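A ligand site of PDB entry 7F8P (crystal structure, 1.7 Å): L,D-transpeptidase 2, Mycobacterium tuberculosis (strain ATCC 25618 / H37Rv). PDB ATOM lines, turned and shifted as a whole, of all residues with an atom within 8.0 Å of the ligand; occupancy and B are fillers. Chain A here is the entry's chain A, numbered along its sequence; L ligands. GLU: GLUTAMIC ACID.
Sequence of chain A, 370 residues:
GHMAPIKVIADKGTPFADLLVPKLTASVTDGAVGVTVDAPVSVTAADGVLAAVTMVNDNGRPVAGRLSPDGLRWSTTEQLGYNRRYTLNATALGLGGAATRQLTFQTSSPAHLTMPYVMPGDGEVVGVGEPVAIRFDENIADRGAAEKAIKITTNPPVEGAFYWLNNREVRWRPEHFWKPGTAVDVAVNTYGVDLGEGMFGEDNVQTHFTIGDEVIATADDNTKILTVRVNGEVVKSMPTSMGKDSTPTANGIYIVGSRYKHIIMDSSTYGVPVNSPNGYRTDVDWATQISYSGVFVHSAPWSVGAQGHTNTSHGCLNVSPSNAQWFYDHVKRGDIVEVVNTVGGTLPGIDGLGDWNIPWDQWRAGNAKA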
ATOM      1  N   ASP A 266     -20.486  -7.293 -16.876  1.00  0.00           N
ATOM      2  CA  ASP A 266     -19.815  -8.533 -16.477  1.00  0.00           C
ATOM      3  C   ASP A 266     -19.147  -9.096 -17.727  1.00  0.00           C
ATOM      4  O   ASP A 266     -19.835  -9.518 -18.653  1.00  0.00           O
ATOM      5  CB  ASP A 266     -20.837  -9.513 -15.897  1.00  0.00           C
ATOM      6  CG  ASP A 266     -20.188 -10.745 -15.288  1.00  0.00           C
ATOM      7  OD1 ASP A 266     -19.254 -11.306 -15.898  1.00  0.00           O
ATOM      8  OD2 ASP A 266     -20.635 -11.172 -14.191  1.00  0.00           O
ATOM      9  N   SER A 267     -17.813  -9.106 -17.745  1.00  0.00           N
ATOM     10  CA  SER A 267     -17.099  -9.518 -18.938  1.00  0.00           C
ATOM     11  C   SER A 267     -17.424 -10.952 -19.331  1.00  0.00           C
ATOM     12  O   SER A 267     -17.312 -11.317 -20.509  1.00  0.00           O
ATOM     13  CB  SER A 267     -15.589  -9.352 -18.759  1.00  0.00           C
ATOM     14  OG  SER A 267     -15.083 -10.216 -17.759  1.00  0.00           O
ATOM     15  N   SER A 268     -17.834 -11.793 -18.368  1.00  0.00           N
ATOM     16  CA  SER A 268     -18.169 -13.167 -18.702  1.00  0.00           C
ATOM     17  C   SER A 268     -19.370 -13.240 -19.629  1.00  0.00           C
ATOM     18  O   SER A 268     -19.518 -14.214 -20.389  1.00  0.00           O
ATOM     19  CB  SER A 268     -18.430 -13.984 -17.435  1.00  0.00           C
ATOM     20  OG  SER A 268     -19.024 -15.242 -17.757  1.00  0.00           O
ATOM     21  N   THR A 269     -20.251 -12.236 -19.576  1.00  0.00           N
ATOM     22  CA  THR A 269     -21.349 -12.154 -20.539  1.00  0.00           C
ATOM     23  C   THR A 269     -20.830 -12.110 -21.972  1.00  0.00           C
ATOM     24  O   THR A 269     -21.486 -12.597 -22.891  1.00  0.00           O
ATOM     25  CB  THR A 269     -22.205 -10.917 -20.263  1.00  0.00           C
ATOM     26  OG1 THR A 269     -22.576 -10.900 -18.881  1.00  0.00           O
ATOM     27  CG2 THR A 269     -23.449 -10.906 -21.135  1.00  0.00           C
ATOM     28  N   GLY A 271     -17.825 -13.371 -23.028  1.00  0.00           N
ATOM     29  CA  GLY A 271     -16.844 -14.414 -23.288  1.00  0.00           C
ATOM     30  C   GLY A 271     -15.502 -14.267 -22.593  1.00  0.00           C
ATOM     31  O   GLY A 271     -14.582 -15.026 -22.908  1.00  0.00           O
ATOM     32  N   VAL A 272     -15.356 -13.337 -21.655  1.00  0.00           N
ATOM     33  CA  VAL A 272     -14.078 -13.066 -21.009  1.00  0.00           C
ATOM     34  C   VAL A 272     -14.232 -13.315 -19.510  1.00  0.00           C
ATOM     35  O   VAL A 272     -14.990 -12.608 -18.836  1.00  0.00           O
ATOM     36  CB  VAL A 272     -13.601 -11.632 -21.262  1.00  0.00           C
ATOM     37  CG1 VAL A 272     -12.277 -11.388 -20.548  1.00  0.00           C
ATOM     38  CG2 VAL A 272     -13.480 -11.362 -22.753  1.00  0.00           C
ATOM     39  N   PRO A 273     -13.507 -14.281 -18.934  1.00  0.00           N
ATOM     40  CA  PRO A 273     -13.631 -14.539 -17.492  1.00  0.00           C
ATOM     41  C   PRO A 273     -13.174 -13.350 -16.651  1.00  0.00           C
ATOM     42  O   PRO A 273     -12.187 -12.689 -16.957  1.00  0.00           O
ATOM     43  CB  PRO A 273     -12.715 -15.751 -17.272  1.00  0.00           C
ATOM     44  CG  PRO A 273     -12.547 -16.368 -18.622  1.00  0.00           C
ATOM     45  CD  PRO A 273     -12.597 -15.227 -19.593  1.00  0.00           C
ATOM     46  N   VAL A 274     -13.918 -13.099 -15.574  1.00  0.00           N
ATOM     47  CA  VAL A 274     -13.690 -11.897 -14.775  1.00  0.00           C
ATOM     48  C   VAL A 274     -12.280 -11.887 -14.201  1.00  0.00           C
ATOM     49  O   VAL A 274     -11.595 -10.846 -14.229  1.00  0.00           O
ATOM     50  CB  VAL A 274     -14.755 -11.784 -13.669  1.00  0.00           C
ATOM     51  CG1 VAL A 274     -14.468 -10.576 -12.776  1.00  0.00           C
ATOM     52  CG2 VAL A 274     -16.155 -11.688 -14.284  1.00  0.00           C
ATOM     53  N   ASN A 275     -11.810 -13.013 -13.677  1.00  0.00           N
ATOM     54  CA  ASN A 275     -10.485 -13.034 -13.078  1.00  0.00           C
ATOM     55  C   ASN A 275      -9.367 -13.145 -14.104  1.00  0.00           C
ATOM     56  O   ASN A 275      -8.193 -13.262 -13.708  1.00  0.00           O
ATOM     57  CB  ASN A 275     -10.364 -14.175 -12.048  1.00  0.00           C
ATOM     58  CG  ASN A 275     -11.536 -14.234 -11.056  1.00  0.00           C
ATOM     59  OD1 ASN A 275     -12.146 -13.212 -10.738  1.00  0.00           O
ATOM     60  ND2 ASN A 275     -11.812 -15.434 -10.546  1.00  0.00           N
ATOM     61  N   SER A 276      -9.681 -13.120 -15.390  1.00  0.00           N
ATOM     62  CA  SER A 276      -8.668 -13.180 -16.444  1.00  0.00           C
ATOM     63  C   SER A 276      -8.074 -11.782 -16.662  1.00  0.00           C
ATOM     64  O   SER A 276      -8.590 -10.791 -16.144  1.00  0.00           O
ATOM     65  CB  SER A 276      -9.281 -13.766 -17.721  1.00  0.00           C
ATOM     66  OG  SER A 276     -10.089 -12.823 -18.400  1.00  0.00           O
ATOM     67  N   GLY A 279     -10.592  -9.403 -17.897  1.00  0.00           N
ATOM     68  CA  GLY A 279     -11.903  -9.529 -17.303  1.00  0.00           C
ATOM     69  C   GLY A 279     -12.225  -8.360 -16.400  1.00  0.00           C
ATOM     70  O   GLY A 279     -11.359  -7.599 -15.982  1.00  0.00           O
ATOM     71  N   TYR A 280     -13.509  -8.231 -16.098  1.00  0.00           N
ATOM     72  CA  TYR A 280     -13.984  -7.153 -15.245  1.00  0.00           C
ATOM     73  C   TYR A 280     -15.400  -7.468 -14.816  1.00  0.00           C
ATOM     74  O   TYR A 280     -16.126  -8.207 -15.489  1.00  0.00           O
ATOM     75  CB  TYR A 280     -13.939  -5.797 -15.952  1.00  0.00           C
ATOM     76  CG  TYR A 280     -14.667  -5.766 -17.285  1.00  0.00           C
ATOM     77  CD1 TYR A 280     -16.059  -5.618 -17.331  1.00  0.00           C
ATOM     78  CD2 TYR A 280     -13.981  -5.878 -18.481  1.00  0.00           C
ATOM     79  CE1 TYR A 280     -16.737  -5.606 -18.537  1.00  0.00           C
ATOM     80  CE2 TYR A 280     -14.652  -5.855 -19.692  1.00  0.00           C
ATOM     81  CZ  TYR A 280     -16.024  -5.717 -19.720  1.00  0.00           C
ATOM     82  OH  TYR A 280     -16.698  -5.681 -20.926  1.00  0.00           O
ATOM     83  N   ARG A 281     -15.793  -6.884 -13.692  1.00  0.00           N
ATOM     84  CA  ARG A 281     -17.188  -6.839 -13.270  1.00  0.00           C
ATOM     85  C   ARG A 281     -17.393  -5.477 -12.614  1.00  0.00           C
ATOM     86  O   ARG A 281     -16.888  -5.228 -11.524  1.00  0.00           O
ATOM     87  CB  ARG A 281     -17.527  -7.986 -12.304  1.00  0.00           C
ATOM     88  CG  ARG A 281     -19.000  -8.199 -12.053  1.00  0.00           C
ATOM     89  CD  ARG A 281     -19.223  -9.461 -11.218  1.00  0.00           C
ATOM     90  NE  ARG A 281     -18.066  -9.647 -10.351  1.00  0.00           N
ATOM     91  CZ  ARG A 281     -17.425 -10.786 -10.172  1.00  0.00           C
ATOM     92  NH1 ARG A 281     -17.806 -11.913 -10.784  1.00  0.00           N
ATOM     93  NH2 ARG A 281     -16.375 -10.797  -9.367  1.00  0.00           N
HETATM   94  N   GLU L   1     -16.696 -15.098 -15.155  1.00  0.00           N
HETATM   95  CA  GLU L   1     -16.079 -16.312 -15.665  1.00  0.00           C
HETATM   96  C   GLU L   1     -17.092 -17.390 -16.002  1.00  0.00           C
HETATM   97  O   GLU L   1     -17.787 -17.893 -15.117  1.00  0.00           O
HETATM   98  CB  GLU L   1     -15.092 -16.820 -14.644  1.00  0.00           C
HETATM   99  CG  GLU L   1     -14.470 -15.642 -13.951  1.00  0.00           C
HETATM  100  CD  GLU L   1     -13.559 -16.041 -12.875  1.00  0.00           C
HETATM  101  OE1 GLU L   1     -12.360 -16.231 -13.166  1.00  0.00           O
HETATM  102  OE2 GLU L   1     -14.033 -16.167 -11.726  1.00  0.00           O
HETATM  103  OXT GLU L   1     -17.228 -17.751 -17.172  1.00  0.00           O
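Residues that only touch the ligand: Pro 273 (3.5 Å).
An oxygen (OE1) of the ligand sits close to the backbone NH (N) of Asn 275. The side-chain amide nitrogen (ND2) of Asn 275 sits at hydrogen-bond distance from an oxygen (OE2) of the ligand, at 2.6 Å. The backbone NH of Val 274 sits close to a nitrogen (N) of the ligand, at 3.4 Å. An oxygen (OXT) of the ligand sits at hydrogen-bond distance from the side-chain hydroxyl (OG) of Ser 268.
The backbone NH (N) of Ser 268 sits at hydrogen-bond distance from the side-chain carboxylate (OD1) of Asp 266, 2.9 Å away. The side-chain hydroxyl (OG) of Ser 276 sits at hydrogen-bond distance from the backbone carbonyl oxygen (O) of Pro 273, at 2.5 Å.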
